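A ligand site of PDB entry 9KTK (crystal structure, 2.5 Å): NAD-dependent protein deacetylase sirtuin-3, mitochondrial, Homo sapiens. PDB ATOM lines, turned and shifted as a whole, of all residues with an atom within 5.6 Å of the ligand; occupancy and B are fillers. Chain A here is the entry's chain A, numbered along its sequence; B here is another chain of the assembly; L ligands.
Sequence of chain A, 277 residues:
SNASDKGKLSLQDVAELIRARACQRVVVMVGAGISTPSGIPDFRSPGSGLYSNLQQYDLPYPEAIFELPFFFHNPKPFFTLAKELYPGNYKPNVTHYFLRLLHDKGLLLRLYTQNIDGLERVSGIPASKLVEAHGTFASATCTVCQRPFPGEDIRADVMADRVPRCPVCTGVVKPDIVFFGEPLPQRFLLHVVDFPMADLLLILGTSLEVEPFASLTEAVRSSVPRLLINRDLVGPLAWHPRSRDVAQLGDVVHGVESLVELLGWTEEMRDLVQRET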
ATOM      1  N   PHE A  43     -30.301 -16.568 -22.410  1.00  0.00           N
ATOM      2  CA  PHE A  43     -29.514 -15.411 -22.837  1.00  0.00           C
ATOM      3  C   PHE A  43     -28.963 -15.536 -24.259  1.00  0.00           C
ATOM      4  O   PHE A  43     -28.462 -14.537 -24.794  1.00  0.00           O
ATOM      5  CB  PHE A  43     -28.365 -15.190 -21.855  1.00  0.00           C
ATOM      6  CG  PHE A  43     -27.287 -16.239 -21.935  1.00  0.00           C
ATOM      7  CD1 PHE A  43     -27.473 -17.515 -21.421  1.00  0.00           C
ATOM      8  CD2 PHE A  43     -26.063 -15.948 -22.567  1.00  0.00           C
ATOM      9  CE1 PHE A  43     -26.468 -18.484 -21.511  1.00  0.00           C
ATOM     10  CE2 PHE A  43     -25.051 -16.886 -22.659  1.00  0.00           C
ATOM     11  CZ  PHE A  43     -25.252 -18.175 -22.133  1.00  0.00           C
ATOM     12  N   ARG A  44     -29.057 -16.703 -24.904  1.00  0.00           N
ATOM     13  CA  ARG A  44     -28.345 -16.891 -26.166  1.00  0.00           C
ATOM     14  C   ARG A  44     -29.167 -16.545 -27.403  1.00  0.00           C
ATOM     15  O   ARG A  44     -28.582 -16.144 -28.411  1.00  0.00           O
ATOM     16  CB  ARG A  44     -27.848 -18.331 -26.272  1.00  0.00           C
ATOM     17  CG  ARG A  44     -26.741 -18.626 -25.297  1.00  0.00           C
ATOM     18  CD  ARG A  44     -26.061 -19.906 -25.672  1.00  0.00           C
ATOM     19  NE  ARG A  44     -26.992 -21.023 -25.556  1.00  0.00           N
ATOM     20  CZ  ARG A  44     -27.061 -22.020 -26.436  1.00  0.00           C
ATOM     21  NH1 ARG A  44     -26.289 -22.037 -27.510  1.00  0.00           N
ATOM     22  NH2 ARG A  44     -27.917 -23.014 -26.229  1.00  0.00           N
ATOM     23  N   GLU A  63     -20.831 -16.207 -24.615  1.00  0.00           N
ATOM     24  CA  GLU A  63     -20.195 -17.011 -23.573  1.00  0.00           C
ATOM     25  C   GLU A  63     -19.299 -16.174 -22.690  1.00  0.00           C
ATOM     26  O   GLU A  63     -19.058 -16.551 -21.542  1.00  0.00           O
ATOM     27  CB  GLU A  63     -19.308 -18.106 -24.169  1.00  0.00           C
ATOM     28  CG  GLU A  63     -19.955 -19.167 -24.957  1.00  0.00           C
ATOM     29  CD  GLU A  63     -19.483 -19.054 -26.370  1.00  0.00           C
ATOM     30  OE1 GLU A  63     -19.921 -18.084 -27.051  1.00  0.00           O
ATOM     31  OE2 GLU A  63     -18.605 -19.852 -26.760  1.00  0.00           O
ATOM     32  N   PHE A  66     -19.234 -16.199 -19.014  1.00  0.00           N
ATOM     33  CA  PHE A  66     -18.698 -17.246 -18.157  1.00  0.00           C
ATOM     34  C   PHE A  66     -17.182 -17.323 -18.222  1.00  0.00           C
ATOM     35  O   PHE A  66     -16.595 -18.401 -18.030  1.00  0.00           O
ATOM     36  CB  PHE A  66     -19.324 -18.591 -18.492  1.00  0.00           C
ATOM     37  CG  PHE A  66     -20.828 -18.553 -18.602  1.00  0.00           C
ATOM     38  CD1 PHE A  66     -21.590 -18.226 -17.511  1.00  0.00           C
ATOM     39  CD2 PHE A  66     -21.457 -18.903 -19.774  1.00  0.00           C
ATOM     40  CE1 PHE A  66     -22.988 -18.228 -17.598  1.00  0.00           C
ATOM     41  CE2 PHE A  66     -22.840 -18.893 -19.873  1.00  0.00           C
ATOM     42  CZ  PHE A  66     -23.610 -18.547 -18.773  1.00  0.00           C
ATOM     43  N   LEU A  81     -27.143 -11.430 -15.808  1.00  0.00           N
ATOM     44  CA  LEU A  81     -27.645 -12.801 -15.960  1.00  0.00           C
ATOM     45  C   LEU A  81     -28.014 -13.397 -14.599  1.00  0.00           C
ATOM     46  O   LEU A  81     -29.037 -14.075 -14.472  1.00  0.00           O
ATOM     47  CB  LEU A  81     -26.630 -13.699 -16.654  1.00  0.00           C
ATOM     48  CG  LEU A  81     -27.185 -15.108 -16.842  1.00  0.00           C
ATOM     49  CD1 LEU A  81     -27.625 -15.323 -18.251  1.00  0.00           C
ATOM     50  CD2 LEU A  81     -26.195 -16.168 -16.430  1.00  0.00           C
ATOM     51  N   LEU A  85     -31.766 -14.714 -12.990  1.00  0.00           N
ATOM     52  CA  LEU A  85     -31.894 -16.145 -12.769  1.00  0.00           C
ATOM     53  C   LEU A  85     -31.919 -16.579 -11.310  1.00  0.00           C
ATOM     54  O   LEU A  85     -32.192 -17.758 -11.047  1.00  0.00           O
ATOM     55  CB  LEU A  85     -30.761 -16.895 -13.488  1.00  0.00           C
ATOM     56  CG  LEU A  85     -30.941 -16.835 -14.997  1.00  0.00           C
ATOM     57  CD1 LEU A  85     -29.847 -17.623 -15.752  1.00  0.00           C
ATOM     58  CD2 LEU A  85     -32.348 -17.265 -15.393  1.00  0.00           C
ATOM     59  N   GLN A 114     -28.054 -29.124 -17.114  1.00  0.00           N
ATOM     60  CA  GLN A 114     -27.252 -27.976 -17.541  1.00  0.00           C
ATOM     61  C   GLN A 114     -27.807 -26.667 -17.020  1.00  0.00           C
ATOM     62  O   GLN A 114     -27.161 -25.627 -17.184  1.00  0.00           O
ATOM     63  CB  GLN A 114     -27.177 -27.864 -19.071  1.00  0.00           C
ATOM     64  CG  GLN A 114     -26.884 -29.145 -19.827  1.00  0.00           C
ATOM     65  CD  GLN A 114     -26.025 -28.911 -21.037  1.00  0.00           C
ATOM     66  OE1 GLN A 114     -24.787 -28.974 -20.961  1.00  0.00           O
ATOM     67  NE2 GLN A 114     -26.661 -28.620 -22.176  1.00  0.00           N
ATOM     68  N   ILE A 116     -29.176 -23.792 -14.307  1.00  0.00           N
ATOM     69  CA  ILE A 116     -28.510 -23.143 -13.182  1.00  0.00           C
ATOM     70  C   ILE A 116     -29.575 -22.353 -12.440  1.00  0.00           C
ATOM     71  O   ILE A 116     -29.274 -21.560 -11.542  1.00  0.00           O
ATOM     72  CB  ILE A 116     -27.333 -22.283 -13.699  1.00  0.00           C
ATOM     73  CG1 ILE A 116     -27.811 -21.076 -14.526  1.00  0.00           C
ATOM     74  CG2 ILE A 116     -26.408 -23.093 -14.573  1.00  0.00           C
ATOM     75  CD1 ILE A 116     -26.815 -19.875 -14.478  1.00  0.00           C
ATOM     76  N   HIS A 134     -23.507 -27.276 -14.750  1.00  0.00           N
ATOM     77  CA  HIS A 134     -23.034 -25.921 -14.895  1.00  0.00           C
ATOM     78  C   HIS A 134     -22.994 -25.178 -13.569  1.00  0.00           C
ATOM     79  O   HIS A 134     -22.997 -23.952 -13.544  1.00  0.00           O
ATOM     80  CB  HIS A 134     -23.889 -25.177 -15.936  1.00  0.00           C
ATOM     81  CG  HIS A 134     -23.620 -25.616 -17.349  1.00  0.00           C
ATOM     82  ND1 HIS A 134     -24.357 -25.165 -18.425  1.00  0.00           N
ATOM     83  CD2 HIS A 134     -22.697 -26.469 -17.850  1.00  0.00           C
ATOM     84  CE1 HIS A 134     -23.900 -25.723 -19.534  1.00  0.00           C
ATOM     85  NE2 HIS A 134     -22.897 -26.518 -19.217  1.00  0.00           N
ATOM     86  N   ILE A 177     -21.451 -20.742 -10.347  1.00  0.00           N
ATOM     87  CA  ILE A 177     -21.747 -21.095 -11.735  1.00  0.00           C
ATOM     88  C   ILE A 177     -20.417 -21.387 -12.429  1.00  0.00           C
ATOM     89  O   ILE A 177     -19.449 -20.620 -12.299  1.00  0.00           O
ATOM     90  CB  ILE A 177     -22.517 -19.946 -12.416  1.00  0.00           C
ATOM     91  CG1 ILE A 177     -23.776 -19.697 -11.586  1.00  0.00           C
ATOM     92  CG2 ILE A 177     -22.863 -20.300 -13.892  1.00  0.00           C
ATOM     93  CD1 ILE A 177     -24.645 -20.928 -11.508  1.00  0.00           C
ATOM     94  N   VAL A 178     -20.346 -22.535 -13.097  1.00  0.00           N
ATOM     95  CA  VAL A 178     -19.076 -22.963 -13.683  1.00  0.00           C
ATOM     96  C   VAL A 178     -18.632 -21.966 -14.743  1.00  0.00           C
ATOM     97  O   VAL A 178     -19.452 -21.480 -15.542  1.00  0.00           O
ATOM     98  CB  VAL A 178     -19.210 -24.395 -14.234  1.00  0.00           C
ATOM     99  CG1 VAL A 178     -18.038 -24.766 -15.076  1.00  0.00           C
ATOM    100  CG2 VAL A 178     -19.390 -25.392 -13.087  1.00  0.00           C
ATOM    101  N   PHE A 179     -17.346 -21.627 -14.730  1.00  0.00           N
ATOM    102  CA  PHE A 179     -16.700 -20.673 -15.611  1.00  0.00           C
ATOM    103  C   PHE A 179     -15.585 -21.365 -16.402  1.00  0.00           C
ATOM    104  O   PHE A 179     -14.945 -22.296 -15.910  1.00  0.00           O
ATOM    105  CB  PHE A 179     -16.056 -19.545 -14.801  1.00  0.00           C
ATOM    106  CG  PHE A 179     -16.859 -18.288 -14.693  1.00  0.00           C
ATOM    107  CD1 PHE A 179     -18.240 -18.319 -14.704  1.00  0.00           C
ATOM    108  CD2 PHE A 179     -16.214 -17.068 -14.494  1.00  0.00           C
ATOM    109  CE1 PHE A 179     -18.978 -17.153 -14.567  1.00  0.00           C
ATOM    110  CE2 PHE A 179     -16.924 -15.871 -14.366  1.00  0.00           C
ATOM    111  CZ  PHE A 179     -18.324 -15.919 -14.401  1.00  0.00           C
ATOM    112  N   PHE A 180     -15.302 -20.871 -17.603  1.00  0.00           N
ATOM    113  CA  PHE A 180     -14.187 -21.405 -18.368  1.00  0.00           C
ATOM    114  C   PHE A 180     -12.887 -21.319 -17.571  1.00  0.00           C
ATOM    115  O   PHE A 180     -12.506 -20.256 -17.057  1.00  0.00           O
ATOM    116  CB  PHE A 180     -14.023 -20.659 -19.696  1.00  0.00           C
ATOM    117  CG  PHE A 180     -15.182 -20.812 -20.649  1.00  0.00           C
ATOM    118  CD1 PHE A 180     -15.401 -22.012 -21.319  1.00  0.00           C
ATOM    119  CD2 PHE A 180     -16.035 -19.738 -20.887  1.00  0.00           C
ATOM    120  CE1 PHE A 180     -16.467 -22.151 -22.194  1.00  0.00           C
ATOM    121  CE2 PHE A 180     -17.095 -19.847 -21.765  1.00  0.00           C
ATOM    122  CZ  PHE A 180     -17.328 -21.048 -22.422  1.00  0.00           C
ATOM    123  N   GLY A 181     -12.194 -22.442 -17.477  1.00  0.00           N
ATOM    124  CA  GLY A 181     -10.979 -22.527 -16.713  1.00  0.00           C
ATOM    125  C   GLY A 181     -11.153 -23.194 -15.369  1.00  0.00           C
ATOM    126  O   GLY A 181     -10.159 -23.610 -14.772  1.00  0.00           O
ATOM    127  N   GLU A 182     -12.381 -23.278 -14.877  1.00  0.00           N
ATOM    128  CA  GLU A 182     -12.622 -23.929 -13.607  1.00  0.00           C
ATOM    129  C   GLU A 182     -12.727 -25.432 -13.800  1.00  0.00           C
ATOM    130  O   GLU A 182     -13.148 -25.898 -14.859  1.00  0.00           O
ATOM    131  CB  GLU A 182     -13.892 -23.408 -12.960  1.00  0.00           C
ATOM    132  CG  GLU A 182     -13.750 -22.073 -12.264  1.00  0.00           C
ATOM    133  CD  GLU A 182     -15.106 -21.455 -11.867  1.00  0.00           C
ATOM    134  OE1 GLU A 182     -16.158 -21.897 -12.391  1.00  0.00           O
ATOM    135  OE2 GLU A 182     -15.109 -20.490 -11.074  1.00  0.00           O
ATOM    136  N   LEU A 184     -14.269 -29.066 -13.716  1.00  0.00           N
ATOM    137  CA  LEU A 184     -15.676 -29.395 -13.849  1.00  0.00           C
ATOM    138  C   LEU A 184     -16.239 -29.846 -12.504  1.00  0.00           C
ATOM    139  O   LEU A 184     -15.491 -30.265 -11.609  1.00  0.00           O
ATOM    140  CB  LEU A 184     -15.878 -30.443 -14.950  1.00  0.00           C
ATOM    141  CG  LEU A 184     -15.642 -31.920 -14.734  1.00  0.00           C
ATOM    142  CD1 LEU A 184     -16.004 -32.682 -16.003  1.00  0.00           C
ATOM    143  CD2 LEU A 184     -14.193 -32.107 -14.481  1.00  0.00           C
ATOM    144  N   VAL A 210     -23.124 -28.459 -25.606  1.00  0.00           N
ATOM    145  CA  VAL A 210     -22.122 -28.168 -24.582  1.00  0.00           C
ATOM    146  C   VAL A 210     -21.601 -29.505 -24.017  1.00  0.00           C
ATOM    147  O   VAL A 210     -22.265 -30.157 -23.216  1.00  0.00           O
ATOM    148  CB  VAL A 210     -22.703 -27.304 -23.458  1.00  0.00           C
ATOM    149  CG1 VAL A 210     -21.606 -26.695 -22.626  1.00  0.00           C
ATOM    150  CG2 VAL A 210     -23.613 -26.214 -24.020  1.00  0.00           C
ATOM    151  N   GLU A 211     -20.380 -29.885 -24.422  1.00  0.00           N
ATOM    152  CA  GLU A 211     -19.723 -31.047 -23.843  1.00  0.00           C
ATOM    153  C   GLU A 211     -18.946 -30.610 -22.594  1.00  0.00           C
ATOM    154  O   GLU A 211     -18.704 -29.414 -22.400  1.00  0.00           O
ATOM    155  CB  GLU A 211     -18.820 -31.717 -24.887  1.00  0.00           C
ATOM    156  CG  GLU A 211     -19.438 -33.012 -25.465  1.00  0.00           C
ATOM    157  CD  GLU A 211     -19.131 -33.168 -26.956  1.00  0.00           C
ATOM    158  OE1 GLU A 211     -18.291 -32.391 -27.475  1.00  0.00           O
ATOM    159  OE2 GLU A 211     -19.734 -34.049 -27.634  1.00  0.00           O
ATOM    160  N   PRO A 212     -18.573 -31.538 -21.690  1.00  0.00           N
ATOM    161  CA  PRO A 212     -18.704 -33.008 -21.738  1.00  0.00           C
ATOM    162  C   PRO A 212     -20.128 -33.521 -21.509  1.00  0.00           C
ATOM    163  O   PRO A 212     -20.382 -34.725 -21.640  1.00  0.00           O
ATOM    164  CB  PRO A 212     -17.711 -33.470 -20.662  1.00  0.00           C
ATOM    165  CG  PRO A 212     -17.623 -32.350 -19.695  1.00  0.00           C
ATOM    166  CD  PRO A 212     -17.975 -31.090 -20.415  1.00  0.00           C
ATOM    167  N   PRO B  60     -10.648 -24.676 -21.565  1.00  0.00           N
ATOM    168  CA  PRO B  60     -11.855 -24.495 -20.748  1.00  0.00           C
ATOM    169  C   PRO B  60     -11.690 -25.254 -19.458  1.00  0.00           C
ATOM    170  O   PRO B  60     -10.937 -24.814 -18.589  1.00  0.00           O
ATOM    171  CB  PRO B  60     -12.986 -25.027 -21.637  1.00  0.00           C
ATOM    172  CG  PRO B  60     -12.315 -25.960 -22.578  1.00  0.00           C
ATOM    173  CD  PRO B  60     -10.900 -25.483 -22.762  1.00  0.00           C
ATOM    174  N   TYR B  61     -12.275 -26.371 -19.314  1.00  0.00           N
ATOM    175  CA  TYR B  61     -12.012 -26.930 -17.987  1.00  0.00           C
ATOM    176  C   TYR B  61     -10.651 -27.634 -17.994  1.00  0.00           C
ATOM    177  O   TYR B  61     -10.256 -28.184 -19.020  1.00  0.00           O
ATOM    178  CB  TYR B  61     -13.125 -27.868 -17.562  1.00  0.00           C
ATOM    179  CG  TYR B  61     -13.488 -28.931 -18.574  1.00  0.00           C
ATOM    180  CD1 TYR B  61     -14.120 -28.622 -19.782  1.00  0.00           C
ATOM    181  CD2 TYR B  61     -13.240 -30.275 -18.291  1.00  0.00           C
ATOM    182  CE1 TYR B  61     -14.471 -29.618 -20.679  1.00  0.00           C
ATOM    183  CE2 TYR B  61     -13.584 -31.272 -19.181  1.00  0.00           C
ATOM    184  CZ  TYR B  61     -14.190 -30.934 -20.369  1.00  0.00           C
ATOM    185  OH  TYR B  61     -14.515 -31.923 -21.235  1.00  0.00           O
HETATM  186  N1  LIG L   1     -21.525 -22.070 -16.753  1.00  0.00           N
HETATM  187  N2  LIG L   1     -20.881 -22.231 -21.541  1.00  0.00           N
HETATM  188  C1  LIG L   1     -21.790 -22.094 -18.100  1.00  0.00           C
HETATM  189  C2  LIG L   1     -19.382 -22.203 -18.891  1.00  0.00           C
HETATM  190  C3  LIG L   1     -18.722 -23.544 -18.932  1.00  0.00           C
HETATM  191  C4  LIG L   1     -19.419 -24.691 -19.255  1.00  0.00           C
HETATM  192  C5  LIG L   1     -18.757 -25.902 -19.287  1.00  0.00           C
HETATM  193  C6  LIG L   1     -16.703 -24.789 -18.671  1.00  0.00           C
HETATM  194  C7  LIG L   1     -21.669 -22.195 -22.620  1.00  0.00           C
HETATM  195  C8  LIG L   1     -21.901 -22.214 -25.027  1.00  0.00           C
HETATM  196  C9  LIG L   1     -23.867 -22.086 -23.649  1.00  0.00           C
HETATM  197  C10 LIG L   1     -26.613 -21.333 -18.314  1.00  0.00           C
HETATM  198  C11 LIG L   1     -17.372 -23.577 -18.646  1.00  0.00           C
HETATM  199  C12 LIG L   1     -21.401 -22.181 -20.326  1.00  0.00           C
HETATM  200  C13 LIG L   1     -21.101 -22.253 -23.919  1.00  0.00           C
HETATM  201  C14 LIG L   1     -23.274 -22.130 -24.888  1.00  0.00           C
HETATM  202  C15 LIG L   1     -23.085 -22.114 -22.470  1.00  0.00           C
HETATM  203  C16 LIG L   1     -22.868 -22.095 -20.157  1.00  0.00           C
HETATM  204  C17 LIG L   1     -24.314 -21.951 -18.060  1.00  0.00           C
HETATM  205  C18 LIG L   1     -23.058 -22.053 -18.687  1.00  0.00           C
HETATM  206  C19 LIG L   1     -17.407 -25.947 -18.988  1.00  0.00           C
HETATM  207  F1  LIG L   1     -16.746 -27.118 -19.016  1.00  0.00           F
HETATM  208  N3  LIG L   1     -20.823 -22.194 -19.086  1.00  0.00           N
HETATM  209  N4  LIG L   1     -23.664 -22.070 -21.230  1.00  0.00           N
HETATM  210  O1  LIG L   1     -25.413 -21.902 -18.835  1.00  0.00           O
HETATM  211  O2  LIG L   1     -24.395 -21.895 -16.845  1.00  0.00           O
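Merely in contact with the ligand: Tyr 61 of chain B (3.1 Å), Phe 66 (3.2 Å), Ile 116 (3.3 Å), Glu 63 (3.5 Å), Phe 180 (3.6 Å), Ile 177 (3.6 Å), Phe 179 (3.6 Å) and Arg 44 (3.7 Å). Hydrophobic or aromatic side chains that line the ligand: Phe 66, Ile 116, His 134, Ile 177, Val 178, Phe 180 and Tyr 61 of chain B. Of the 21 residues printed, 10 come within 4 Å of the ligand.
ND1 of His 134 sits close to O1 of the ligand, at 3.5 Å. O of Val 178 is in hydrogen-bond range of N1 of the ligand (2.5 Å).
The backbone NH (N) of Val 178 sits at hydrogen-bond distance from the backbone carbonyl oxygen (O) of His 134 (3.0 Å). The backbone NH (N) of Phe 180 sits at hydrogen-bond distance from the backbone carbonyl oxygen (O) of Phe 66 (2.8 Å). A ring nitrogen (ND1) of His 134 lies within hydrogen-bond range of the backbone carbonyl oxygen of Gln 114 (3.1 Å). The backbone NH (N) of Phe 179 is in hydrogen-bond range of the side-chain carboxylate (OE1) of Glu 182, 2.6 Å away.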
